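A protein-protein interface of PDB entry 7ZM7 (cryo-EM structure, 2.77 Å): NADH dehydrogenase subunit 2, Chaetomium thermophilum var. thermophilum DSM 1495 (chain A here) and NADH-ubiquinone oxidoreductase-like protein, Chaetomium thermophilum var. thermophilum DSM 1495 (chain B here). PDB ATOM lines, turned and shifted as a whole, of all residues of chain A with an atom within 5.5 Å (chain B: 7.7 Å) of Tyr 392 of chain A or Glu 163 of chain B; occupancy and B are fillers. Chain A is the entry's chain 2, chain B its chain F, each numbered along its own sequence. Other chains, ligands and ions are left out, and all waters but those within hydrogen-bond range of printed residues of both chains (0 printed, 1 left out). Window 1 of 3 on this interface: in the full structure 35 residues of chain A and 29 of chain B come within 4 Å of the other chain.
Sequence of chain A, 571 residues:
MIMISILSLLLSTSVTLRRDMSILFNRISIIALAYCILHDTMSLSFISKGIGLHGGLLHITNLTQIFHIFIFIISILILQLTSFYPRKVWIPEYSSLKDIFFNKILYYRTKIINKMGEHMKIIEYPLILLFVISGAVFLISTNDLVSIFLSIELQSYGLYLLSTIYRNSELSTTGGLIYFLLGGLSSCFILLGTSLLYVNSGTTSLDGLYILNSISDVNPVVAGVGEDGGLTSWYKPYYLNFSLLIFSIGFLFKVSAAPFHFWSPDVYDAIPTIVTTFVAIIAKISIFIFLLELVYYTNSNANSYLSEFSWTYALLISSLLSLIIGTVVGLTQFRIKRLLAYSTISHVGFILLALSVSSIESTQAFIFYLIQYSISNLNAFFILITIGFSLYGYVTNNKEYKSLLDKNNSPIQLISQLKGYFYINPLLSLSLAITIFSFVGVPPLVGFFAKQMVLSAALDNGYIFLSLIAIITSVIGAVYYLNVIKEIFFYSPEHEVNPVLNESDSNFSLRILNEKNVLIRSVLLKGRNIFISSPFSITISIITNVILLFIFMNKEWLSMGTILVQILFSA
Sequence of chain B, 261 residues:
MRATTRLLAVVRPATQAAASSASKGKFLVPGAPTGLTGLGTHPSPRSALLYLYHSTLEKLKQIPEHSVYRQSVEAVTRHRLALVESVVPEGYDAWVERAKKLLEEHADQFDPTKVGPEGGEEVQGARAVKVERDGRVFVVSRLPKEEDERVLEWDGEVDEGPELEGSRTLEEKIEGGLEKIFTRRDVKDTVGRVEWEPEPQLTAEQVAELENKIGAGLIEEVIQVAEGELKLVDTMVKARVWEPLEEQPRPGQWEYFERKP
NZ of Lys 111 of chain A is in salt-bridge range of OE2 of Glu 163 of chain B (2.6 Å). N of Glu 165 of chain B is in hydrogen-bond range of OD1 of Asn 408 of chain A, at 2.9 Å. The side-chain carboxylate of Glu 165 of chain B lies within salt-bridge range of the guanidinium group of Arg 87 of chain A (3.2 Å). The side-chain carboxylate (OE2) of Glu 160 of chain B lies within salt-bridge range of the side-chain amino group (NZ) of Lys 111 of chain A (3.4 Å). O of Tyr 392 of chain A sits at hydrogen-bond distance from NZ of Lys 173 of chain B (2.7 Å). The side-chain amide oxygen (OD1) of Asn 408 of chain A is in hydrogen-bond range of the guanidinium group (NH2) of Arg 168 of chain B (2.8 Å). The backbone carbonyl oxygen of Glu 163 of chain B lies within hydrogen-bond range of the side-chain amide nitrogen of Asn 408 of chain A. OD1 of Asn 114 of chain A sits at hydrogen-bond distance from N of Glu 163 of chain B (3.3 Å). OE2 of Glu 165 of chain B is in hydrogen-bond range of ND2 of Asn 114 of chain A. The side-chain hydroxyl (OH) of Tyr 392 of chain A lies within hydrogen-bond range of the side-chain carboxylate (OE1) of Glu 163 of chain B (2.8 Å).
O of Gly 176 of chain B touches NZ of Lys 111 of chain A, at 3.6 Å. Ile 181 of chain B touches Lys 111 of chain A. Ile 181 of chain B touches Ile 112 of chain A (CD1 to CD1, 3.5 Å). Phe 389 of chain A touches Glu 165 of chain B. Tyr 392 of chain A touches Leu 164 of chain B (CD1 to O, 3.98 Å). Tyr 392 of chain A touches Glu 165 of chain B (CD1 to OE2, 3.7 Å). Asn 408 of chain A touches Leu 164 of chain B. Lys 173 of chain B touches Asn 498 of chain A. Asn 498 of chain A touches Leu 178 of chain B. CD2 of Leu 501 of chain A touches CD2 of Leu 178 of chain B, 3.5 Å away.
Of the printed residues of chain B, Tyr 392 of chain A touches Glu 163, Leu 164, Glu 165, Lys 173 and Ile 181. Printed residues of chain A within 4 Å of Glu 160 of chain B: Lys 111. Printed residues of chain B within 4 Å of Asn 408 of chain A: Glu 163 (3.4 Å), Leu 164 (3.8 Å), Glu 165 (2.9 Å) and Arg 168 (2.8 Å). Of the printed residues of chain A, Ile 181 of chain B touches Lys 111 (3.8 Å), Ile 112 (3.5 Å) and Tyr 392 (3.5 Å). Of the printed residues of chain A, Leu 164 of chain B touches Tyr 392 (3.98 Å) and Asn 408 (3.8 Å). Gly 117 of chain A touches none of the printed residues of chain B. The nearest printed residue of chain A that does not touch Lys 173 of chain B is Tyr 394 of chain A (4.02 Å).
The side-chain amide oxygen of Asn 114 of chain A sits close to the backbone NH of Gly 117 of chain A, 3.5 Å away. The backbone carbonyl oxygen (O) of Ile 112 of chain A lies within hydrogen-bond range of the guanidinium group (NE) of Arg 87 of chain A, 3.0 Å away. O of Gly 393 of chain A is in hydrogen-bond range of N of Asn 498 of chain A. The side-chain hydroxyl (OH) of Tyr 392 of chain A sits at hydrogen-bond distance from the backbone carbonyl oxygen (O) of Lys 111 of chain A. The backbone carbonyl oxygen (O) of Lys 173 of chain B sits at hydrogen-bond distance from the backbone NH (N) of Leu 178 of chain B, at 3.2 Å. The guanidinium group of Arg 168 of chain B lies within hydrogen-bond range of the backbone carbonyl oxygen of Glu 165 of chain B (2.9 Å).
Hydrophobic or aromatic side chains of chain A within 4 Å of the printed part of chain B: Ile 112, Phe 389, Tyr 392 and Leu 501. Along chain A the printed residues that touch a printed residue of chain B span positions 87 to 501. Among the printed residues, 22 pairs touch across the chains.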
ATOM      1  N   ARG A  87       1.795 -20.943  18.051  1.00  0.00           N
ATOM      2  CA  ARG A  87       2.500 -21.910  17.171  1.00  0.00           C
ATOM      3  C   ARG A  87       3.432 -22.790  18.000  1.00  0.00           C
ATOM      4  O   ARG A  87       3.753 -22.411  19.127  1.00  0.00           O
ATOM      5  CB  ARG A  87       3.305 -21.186  16.091  1.00  0.00           C
ATOM      6  CG  ARG A  87       2.472 -20.377  15.111  1.00  0.00           C
ATOM      7  CD  ARG A  87       3.303 -19.406  14.295  1.00  0.00           C
ATOM      8  NE  ARG A  87       3.884 -18.319  15.067  1.00  0.00           N
ATOM      9  CZ  ARG A  87       3.287 -17.158  15.314  1.00  0.00           C
ATOM     10  NH1 ARG A  87       2.069 -16.923  14.860  1.00  0.00           N
ATOM     11  NH2 ARG A  87       3.908 -16.232  16.019  1.00  0.00           N
ATOM     12  N   THR A 110      11.266 -17.502  21.534  1.00  0.00           N
ATOM     13  CA  THR A 110      10.532 -16.223  21.683  1.00  0.00           C
ATOM     14  C   THR A 110       9.883 -15.768  20.372  1.00  0.00           C
ATOM     15  O   THR A 110       8.685 -15.508  20.391  1.00  0.00           O
ATOM     16  CB  THR A 110      11.471 -15.146  22.245  1.00  0.00           C
ATOM     17  OG1 THR A 110      11.929 -15.587  23.519  1.00  0.00           O
ATOM     18  CG2 THR A 110      10.822 -13.788  22.358  1.00  0.00           C
ATOM     19  N   LYS A 111      10.621 -15.667  19.280  1.00  0.00           N
ATOM     20  CA  LYS A 111      10.016 -15.125  18.069  1.00  0.00           C
ATOM     21  C   LYS A 111       9.177 -16.149  17.331  1.00  0.00           C
ATOM     22  O   LYS A 111       8.294 -15.772  16.558  1.00  0.00           O
ATOM     23  CB  LYS A 111      11.080 -14.570  17.136  1.00  0.00           C
ATOM     24  CG  LYS A 111      11.679 -13.286  17.611  1.00  0.00           C
ATOM     25  CD  LYS A 111      12.753 -12.836  16.664  1.00  0.00           C
ATOM     26  CE  LYS A 111      12.311 -11.596  15.908  1.00  0.00           C
ATOM     27  NZ  LYS A 111      11.818 -10.544  16.834  1.00  0.00           N
ATOM     28  N   ILE A 112       9.436 -17.435  17.541  1.00  0.00           N
ATOM     29  CA  ILE A 112       8.585 -18.461  16.954  1.00  0.00           C
ATOM     30  C   ILE A 112       7.218 -18.469  17.620  1.00  0.00           C
ATOM     31  O   ILE A 112       6.189 -18.495  16.944  1.00  0.00           O
ATOM     32  CB  ILE A 112       9.262 -19.841  17.039  1.00  0.00           C
ATOM     33  CG1 ILE A 112      10.608 -19.818  16.333  1.00  0.00           C
ATOM     34  CG2 ILE A 112       8.371 -20.904  16.446  1.00  0.00           C
ATOM     35  CD1 ILE A 112      10.553 -19.251  14.989  1.00  0.00           C
ATOM     36  N   ASN A 114       5.862 -16.175  19.781  1.00  0.00           N
ATOM     37  CA  ASN A 114       5.292 -14.877  20.135  1.00  0.00           C
ATOM     38  C   ASN A 114       5.073 -14.790  21.645  1.00  0.00           C
ATOM     39  O   ASN A 114       3.986 -14.482  22.128  1.00  0.00           O
ATOM     40  CB  ASN A 114       3.989 -14.636  19.362  1.00  0.00           C
ATOM     41  CG  ASN A 114       3.586 -13.191  19.322  1.00  0.00           C
ATOM     42  OD1 ASN A 114       4.334 -12.311  19.711  1.00  0.00           O
ATOM     43  ND2 ASN A 114       2.396 -12.939  18.828  1.00  0.00           N
ATOM     44  N   GLY A 117       3.764 -11.629  23.055  1.00  0.00           N
ATOM     45  CA  GLY A 117       2.625 -11.058  22.368  1.00  0.00           C
ATOM     46  C   GLY A 117       1.642 -10.403  23.322  1.00  0.00           C
ATOM     47  O   GLY A 117       1.607 -10.684  24.519  1.00  0.00           O
ATOM     48  N   GLY A 388      -4.947 -16.300  11.119  1.00  0.00           N
ATOM     49  CA  GLY A 388      -4.122 -15.117  11.399  1.00  0.00           C
ATOM     50  C   GLY A 388      -2.733 -15.513  11.852  1.00  0.00           C
ATOM     51  O   GLY A 388      -1.762 -14.922  11.355  1.00  0.00           O
ATOM     52  N   PHE A 389      -2.642 -16.467  12.776  1.00  0.00           N
ATOM     53  CA  PHE A 389      -1.339 -16.932  13.305  1.00  0.00           C
ATOM     54  C   PHE A 389      -0.549 -17.690  12.232  1.00  0.00           C
ATOM     55  O   PHE A 389       0.689 -17.701  12.321  1.00  0.00           O
ATOM     56  CB  PHE A 389      -1.551 -17.670  14.623  1.00  0.00           C
ATOM     57  CG  PHE A 389      -1.972 -16.782  15.764  1.00  0.00           C
ATOM     58  CD1 PHE A 389      -1.389 -15.539  15.948  1.00  0.00           C
ATOM     59  CD2 PHE A 389      -2.938 -17.193  16.667  1.00  0.00           C
ATOM     60  CE1 PHE A 389      -1.770 -14.724  17.002  1.00  0.00           C
ATOM     61  CE2 PHE A 389      -3.317 -16.378  17.720  1.00  0.00           C
ATOM     62  CZ  PHE A 389      -2.735 -15.145  17.885  1.00  0.00           C
ATOM     63  N   SER A 390      -1.226 -18.332  11.284  1.00  0.00           N
ATOM     64  CA  SER A 390      -0.598 -19.141  10.207  1.00  0.00           C
ATOM     65  C   SER A 390       0.254 -18.298   9.262  1.00  0.00           C
ATOM     66  O   SER A 390       1.275 -18.809   8.801  1.00  0.00           O
ATOM     67  CB  SER A 390      -1.665 -19.852   9.439  1.00  0.00           C
ATOM     68  OG  SER A 390      -2.235 -18.987   8.475  1.00  0.00           O
ATOM     69  N   LEU A 391      -0.130 -17.050   9.011  1.00  0.00           N
ATOM     70  CA  LEU A 391       0.550 -16.193   7.999  1.00  0.00           C
ATOM     71  C   LEU A 391       1.875 -15.642   8.527  1.00  0.00           C
ATOM     72  O   LEU A 391       2.469 -14.821   7.844  1.00  0.00           O
ATOM     73  CB  LEU A 391      -0.392 -15.064   7.581  1.00  0.00           C
ATOM     74  CG  LEU A 391      -1.686 -15.493   6.895  1.00  0.00           C
ATOM     75  CD1 LEU A 391      -2.475 -14.276   6.440  1.00  0.00           C
ATOM     76  CD2 LEU A 391      -1.395 -16.408   5.718  1.00  0.00           C
ATOM     77  N   TYR A 392       2.305 -16.077   9.707  1.00  0.00           N
ATOM     78  CA  TYR A 392       3.611 -15.637  10.250  1.00  0.00           C
ATOM     79  C   TYR A 392       4.730 -16.033   9.281  1.00  0.00           C
ATOM     80  O   TYR A 392       5.669 -15.256   9.115  1.00  0.00           O
ATOM     81  CB  TYR A 392       3.808 -16.178  11.670  1.00  0.00           C
ATOM     82  CG  TYR A 392       5.128 -15.828  12.306  1.00  0.00           C
ATOM     83  CD1 TYR A 392       5.322 -14.605  12.920  1.00  0.00           C
ATOM     84  CD2 TYR A 392       6.186 -16.723  12.293  1.00  0.00           C
ATOM     85  CE1 TYR A 392       6.534 -14.273  13.501  1.00  0.00           C
ATOM     86  CE2 TYR A 392       7.404 -16.409  12.869  1.00  0.00           C
ATOM     87  CZ  TYR A 392       7.578 -15.179  13.475  1.00  0.00           C
ATOM     88  OH  TYR A 392       8.778 -14.864  14.043  1.00  0.00           O
ATOM     89  N   GLY A 393       4.643 -17.207   8.670  1.00  0.00           N
ATOM     90  CA  GLY A 393       5.645 -17.616   7.669  1.00  0.00           C
ATOM     91  C   GLY A 393       5.283 -17.207   6.253  1.00  0.00           C
ATOM     92  O   GLY A 393       5.820 -17.810   5.317  1.00  0.00           O
ATOM     93  N   TYR A 394       4.390 -16.234   6.090  1.00  0.00           N
ATOM     94  CA  TYR A 394       3.992 -15.772   4.772  1.00  0.00           C
ATOM     95  C   TYR A 394       4.202 -14.270   4.685  1.00  0.00           C
ATOM     96  O   TYR A 394       4.292 -13.579   5.697  1.00  0.00           O
ATOM     97  CB  TYR A 394       2.530 -16.131   4.465  1.00  0.00           C
ATOM     98  CG  TYR A 394       2.350 -17.578   4.102  1.00  0.00           C
ATOM     99  CD1 TYR A 394       2.458 -18.561   5.056  1.00  0.00           C
ATOM    100  CD2 TYR A 394       2.088 -17.957   2.805  1.00  0.00           C
ATOM    101  CE1 TYR A 394       2.321 -19.883   4.728  1.00  0.00           C
ATOM    102  CE2 TYR A 394       1.938 -19.279   2.471  1.00  0.00           C
ATOM    103  CZ  TYR A 394       2.059 -20.232   3.434  1.00  0.00           C
ATOM    104  OH  TYR A 394       1.911 -21.548   3.122  1.00  0.00           O
ATOM    105  N   ASN A 408      -2.225  -6.444  14.573  1.00  0.00           N
ATOM    106  CA  ASN A 408      -1.777  -7.458  15.561  1.00  0.00           C
ATOM    107  C   ASN A 408      -2.969  -7.927  16.391  1.00  0.00           C
ATOM    108  O   ASN A 408      -2.978  -9.096  16.789  1.00  0.00           O
ATOM    109  CB  ASN A 408      -0.625  -6.945  16.423  1.00  0.00           C
ATOM    110  CG  ASN A 408       0.725  -7.082  15.755  1.00  0.00           C
ATOM    111  OD1 ASN A 408       0.814  -7.497  14.606  1.00  0.00           O
ATOM    112  ND2 ASN A 408       1.781  -6.739  16.470  1.00  0.00           N
ATOM    113  N   ASN A 498       7.367 -16.811   3.035  1.00  0.00           N
ATOM    114  CA  ASN A 498       8.504 -15.971   3.342  1.00  0.00           C
ATOM    115  C   ASN A 498       9.747 -16.571   2.704  1.00  0.00           C
ATOM    116  O   ASN A 498      10.029 -17.753   2.917  1.00  0.00           O
ATOM    117  CB  ASN A 498       8.667 -15.868   4.839  1.00  0.00           C
ATOM    118  CG  ASN A 498       9.333 -14.607   5.255  1.00  0.00           C
ATOM    119  OD1 ASN A 498      10.083 -14.010   4.495  1.00  0.00           O
ATOM    120  ND2 ASN A 498       9.044 -14.167   6.470  1.00  0.00           N
ATOM    121  N   LEU A 501      12.634 -17.671   5.492  1.00  0.00           N
ATOM    122  CA  LEU A 501      12.400 -18.871   6.301  1.00  0.00           C
ATOM    123  C   LEU A 501      12.982 -20.119   5.659  1.00  0.00           C
ATOM    124  O   LEU A 501      13.487 -20.998   6.367  1.00  0.00           O
ATOM    125  CB  LEU A 501      10.904 -19.078   6.540  1.00  0.00           C
ATOM    126  CG  LEU A 501      10.218 -18.435   7.747  1.00  0.00           C
ATOM    127  CD1 LEU A 501      10.744 -19.049   9.023  1.00  0.00           C
ATOM    128  CD2 LEU A 501      10.445 -16.960   7.761  1.00  0.00           C
ATOM    129  N   ASP B 159      12.430  -7.236  25.992  1.00  0.00           N
ATOM    130  CA  ASP B 159      11.198  -7.247  25.211  1.00  0.00           C
ATOM    131  C   ASP B 159      11.353  -6.276  24.050  1.00  0.00           C
ATOM    132  O   ASP B 159      11.305  -5.060  24.232  1.00  0.00           O
ATOM    133  CB  ASP B 159      10.006  -6.884  26.086  1.00  0.00           C
ATOM    134  CG  ASP B 159       8.744  -6.633  25.282  1.00  0.00           C
ATOM    135  OD1 ASP B 159       8.533  -7.316  24.261  1.00  0.00           O
ATOM    136  OD2 ASP B 159       7.964  -5.741  25.674  1.00  0.00           O
ATOM    137  N   GLU B 160      11.549  -6.820  22.852  1.00  0.00           N
ATOM    138  CA  GLU B 160      11.550  -6.025  21.633  1.00  0.00           C
ATOM    139  C   GLU B 160      10.149  -5.645  21.181  1.00  0.00           C
ATOM    140  O   GLU B 160      10.007  -4.860  20.240  1.00  0.00           O
ATOM    141  CB  GLU B 160      12.256  -6.794  20.516  1.00  0.00           C
ATOM    142  CG  GLU B 160      12.793  -5.932  19.390  1.00  0.00           C
ATOM    143  CD  GLU B 160      12.901  -6.700  18.087  1.00  0.00           C
ATOM    144  OE1 GLU B 160      12.523  -6.148  17.029  1.00  0.00           O
ATOM    145  OE2 GLU B 160      13.359  -7.860  18.124  1.00  0.00           O
ATOM    146  N   GLY B 161       9.118  -6.190  21.809  1.00  0.00           N
ATOM    147  CA  GLY B 161       7.765  -5.967  21.375  1.00  0.00           C
ATOM    148  C   GLY B 161       7.137  -7.257  20.908  1.00  0.00           C
ATOM    149  O   GLY B 161       7.761  -8.322  20.934  1.00  0.00           O
ATOM    150  N   PRO B 162       5.875  -7.197  20.506  1.00  0.00           N
ATOM    151  CA  PRO B 162       5.255  -8.364  19.890  1.00  0.00           C
ATOM    152  C   PRO B 162       5.761  -8.564  18.476  1.00  0.00           C
ATOM    153  O   PRO B 162       6.187  -7.626  17.803  1.00  0.00           O
ATOM    154  CB  PRO B 162       3.761  -8.027  19.909  1.00  0.00           C
ATOM    155  CG  PRO B 162       3.628  -6.890  20.830  1.00  0.00           C
ATOM    156  CD  PRO B 162       4.898  -6.132  20.738  1.00  0.00           C
ATOM    157  N   GLU B 163       5.728  -9.814  18.038  1.00  0.00           N
ATOM    158  CA  GLU B 163       6.007 -10.114  16.650  1.00  0.00           C
ATOM    159  C   GLU B 163       4.949  -9.495  15.753  1.00  0.00           C
ATOM    160  O   GLU B 163       3.769  -9.442  16.104  1.00  0.00           O
ATOM    161  CB  GLU B 163       6.057 -11.621  16.433  1.00  0.00           C
ATOM    162  CG  GLU B 163       7.233 -12.294  17.096  1.00  0.00           C
ATOM    163  CD  GLU B 163       8.547 -11.939  16.406  1.00  0.00           C
ATOM    164  OE1 GLU B 163       8.733 -12.303  15.221  1.00  0.00           O
ATOM    165  OE2 GLU B 163       9.370 -11.260  17.045  1.00  0.00           O
ATOM    166  N   LEU B 164       5.381  -9.029  14.581  1.00  0.00           N
ATOM    167  CA  LEU B 164       4.393  -8.549  13.582  1.00  0.00           C
ATOM    168  C   LEU B 164       3.538  -9.754  13.209  1.00  0.00           C
ATOM    169  O   LEU B 164       4.121 -10.810  12.921  1.00  0.00           O
ATOM    170  CB  LEU B 164       5.143  -8.020  12.356  1.00  0.00           C
ATOM    171  CG  LEU B 164       6.135  -6.893  12.623  1.00  0.00           C
ATOM    172  CD1 LEU B 164       6.747  -6.414  11.322  1.00  0.00           C
ATOM    173  CD2 LEU B 164       5.460  -5.739  13.346  1.00  0.00           C
ATOM    174  N   GLU B 165       2.220  -9.589  13.164  1.00  0.00           N
ATOM    175  CA  GLU B 165       1.303 -10.694  12.842  1.00  0.00           C
ATOM    176  C   GLU B 165       0.419 -10.196  11.706  1.00  0.00           C
ATOM    177  O   GLU B 165       0.364  -8.982  11.506  1.00  0.00           O
ATOM    178  CB  GLU B 165       0.460 -11.083  14.057  1.00  0.00           C
ATOM    179  CG  GLU B 165       1.261 -11.684  15.199  1.00  0.00           C
ATOM    180  CD  GLU B 165       1.989 -12.993  14.937  1.00  0.00           C
ATOM    181  OE1 GLU B 165       1.451 -13.844  14.196  1.00  0.00           O
ATOM    182  OE2 GLU B 165       3.095 -13.158  15.479  1.00  0.00           O
ATOM    183  N   GLY B 166      -0.227 -11.111  10.990  1.00  0.00           N
ATOM    184  CA  GLY B 166      -1.169 -10.696   9.949  1.00  0.00           C
ATOM    185  C   GLY B 166      -0.515 -10.633   8.597  1.00  0.00           C
ATOM    186  O   GLY B 166       0.570 -11.221   8.429  1.00  0.00           O
ATOM    187  N   SER B 167      -1.191  -9.989   7.651  1.00  0.00           N
ATOM    188  CA  SER B 167      -0.616  -9.827   6.304  1.00  0.00           C
ATOM    189  C   SER B 167       0.472  -8.767   6.427  1.00  0.00           C
ATOM    190  O   SER B 167       0.142  -7.621   6.754  1.00  0.00           O
ATOM    191  CB  SER B 167      -1.694  -9.418   5.363  1.00  0.00           C
ATOM    192  OG  SER B 167      -2.816 -10.275   5.483  1.00  0.00           O
ATOM    193  N   ARG B 168       1.718  -9.138   6.147  1.00  0.00           N
ATOM    194  CA  ARG B 168       2.874  -8.220   6.290  1.00  0.00           C
ATOM    195  C   ARG B 168       3.798  -8.417   5.096  1.00  0.00           C
ATOM    196  O   ARG B 168       3.758  -9.499   4.528  1.00  0.00           O
ATOM    197  CB  ARG B 168       3.643  -8.575   7.567  1.00  0.00           C
ATOM    198  CG  ARG B 168       2.861  -8.420   8.863  1.00  0.00           C
ATOM    199  CD  ARG B 168       2.855  -6.987   9.341  1.00  0.00           C
ATOM    200  NE  ARG B 168       2.207  -6.882  10.636  1.00  0.00           N
ATOM    201  CZ  ARG B 168       2.173  -5.781  11.369  1.00  0.00           C
ATOM    202  NH1 ARG B 168       2.758  -4.681  10.933  1.00  0.00           N
ATOM    203  NH2 ARG B 168       1.554  -5.784  12.533  1.00  0.00           N
ATOM    204  N   LYS B 173       8.978  -7.522   7.644  1.00  0.00           N
ATOM    205  CA  LYS B 173       9.412  -8.625   8.498  1.00  0.00           C
ATOM    206  C   LYS B 173      10.903  -8.543   8.809  1.00  0.00           C
ATOM    207  O   LYS B 173      11.330  -8.884   9.916  1.00  0.00           O
ATOM    208  CB  LYS B 173       9.075  -9.966   7.845  1.00  0.00           C
ATOM    209  CG  LYS B 173       7.607 -10.141   7.485  1.00  0.00           C
ATOM    210  CD  LYS B 173       6.783 -10.639   8.654  1.00  0.00           C
ATOM    211  CE  LYS B 173       6.640 -12.153   8.632  1.00  0.00           C
ATOM    212  NZ  LYS B 173       5.717 -12.664   9.690  1.00  0.00           N
ATOM    213  N   GLY B 176      11.518  -5.999  11.292  1.00  0.00           N
ATOM    214  CA  GLY B 176      10.999  -6.512  12.542  1.00  0.00           C
ATOM    215  C   GLY B 176      11.881  -7.527  13.224  1.00  0.00           C
ATOM    216  O   GLY B 176      11.570  -7.955  14.338  1.00  0.00           O
ATOM    217  N   GLY B 177      12.971  -7.924  12.571  1.00  0.00           N
ATOM    218  CA  GLY B 177      13.983  -8.741  13.197  1.00  0.00           C
ATOM    219  C   GLY B 177      13.921 -10.223  12.923  1.00  0.00           C
ATOM    220  O   GLY B 177      14.530 -10.997  13.665  1.00  0.00           O
ATOM    221  N   LEU B 178      13.225 -10.646  11.870  1.00  0.00           N
ATOM    222  CA  LEU B 178      12.908 -12.061  11.723  1.00  0.00           C
ATOM    223  C   LEU B 178      14.174 -12.897  11.609  1.00  0.00           C
ATOM    224  O   LEU B 178      14.236 -14.024  12.112  1.00  0.00           O
ATOM    225  CB  LEU B 178      12.014 -12.266  10.511  1.00  0.00           C
ATOM    226  CG  LEU B 178      11.419 -13.650  10.299  1.00  0.00           C
ATOM    227  CD1 LEU B 178      10.140 -13.478   9.520  1.00  0.00           C
ATOM    228  CD2 LEU B 178      12.339 -14.607   9.600  1.00  0.00           C
ATOM    229  N   GLU B 179      15.202 -12.353  10.967  1.00  0.00           N
ATOM    230  CA  GLU B 179      16.438 -13.089  10.763  1.00  0.00           C
ATOM    231  C   GLU B 179      17.178 -13.361  12.067  1.00  0.00           C
ATOM    232  O   GLU B 179      18.110 -14.171  12.083  1.00  0.00           O
ATOM    233  CB  GLU B 179      17.330 -12.320   9.791  1.00  0.00           C
ATOM    234  CG  GLU B 179      17.891 -11.013  10.345  1.00  0.00           C
ATOM    235  CD  GLU B 179      16.939  -9.834  10.189  1.00  0.00           C
ATOM    236  OE1 GLU B 179      15.738 -10.050   9.928  1.00  0.00           O
ATOM    237  OE2 GLU B 179      17.397  -8.682  10.331  1.00  0.00           O
ATOM    238  N   ILE B 181      15.921 -15.037  14.391  1.00  0.00           N
ATOM    239  CA  ILE B 181      15.583 -16.400  14.794  1.00  0.00           C
ATOM    240  C   ILE B 181      16.774 -17.319  14.600  1.00  0.00           C
ATOM    241  O   ILE B 181      17.088 -18.146  15.460  1.00  0.00           O
ATOM    242  CB  ILE B 181      14.351 -16.920  14.036  1.00  0.00           C
ATOM    243  CG1 ILE B 181      13.124 -16.097  14.381  1.00  0.00           C
ATOM    244  CG2 ILE B 181      14.109 -18.369  14.360  1.00  0.00           C
ATOM    245  CD1 ILE B 181      11.950 -16.361  13.532  1.00  0.00           C
ATOM    246  N   ARG B 184      20.027 -15.942  17.477  1.00  0.00           N
ATOM    247  CA  ARG B 184      20.093 -15.977  18.923  1.00  0.00           C
ATOM    248  C   ARG B 184      19.991 -17.405  19.436  1.00  0.00           C
ATOM    249  O   ARG B 184      19.713 -18.343  18.696  1.00  0.00           O
ATOM    250  CB  ARG B 184      18.993 -15.140  19.580  1.00  0.00           C
ATOM    251  CG  ARG B 184      19.062 -13.647  19.408  1.00  0.00           C
ATOM    252  CD  ARG B 184      17.899 -13.058  20.170  1.00  0.00           C
ATOM    253  NE  ARG B 184      17.814 -11.608  20.147  1.00  0.00           N
ATOM    254  CZ  ARG B 184      17.134 -10.922  19.250  1.00  0.00           C
ATOM    255  NH1 ARG B 184      16.428 -11.568  18.344  1.00  0.00           N
ATOM    256  NH2 ARG B 184      17.108  -9.600  19.292  1.00  0.00           N
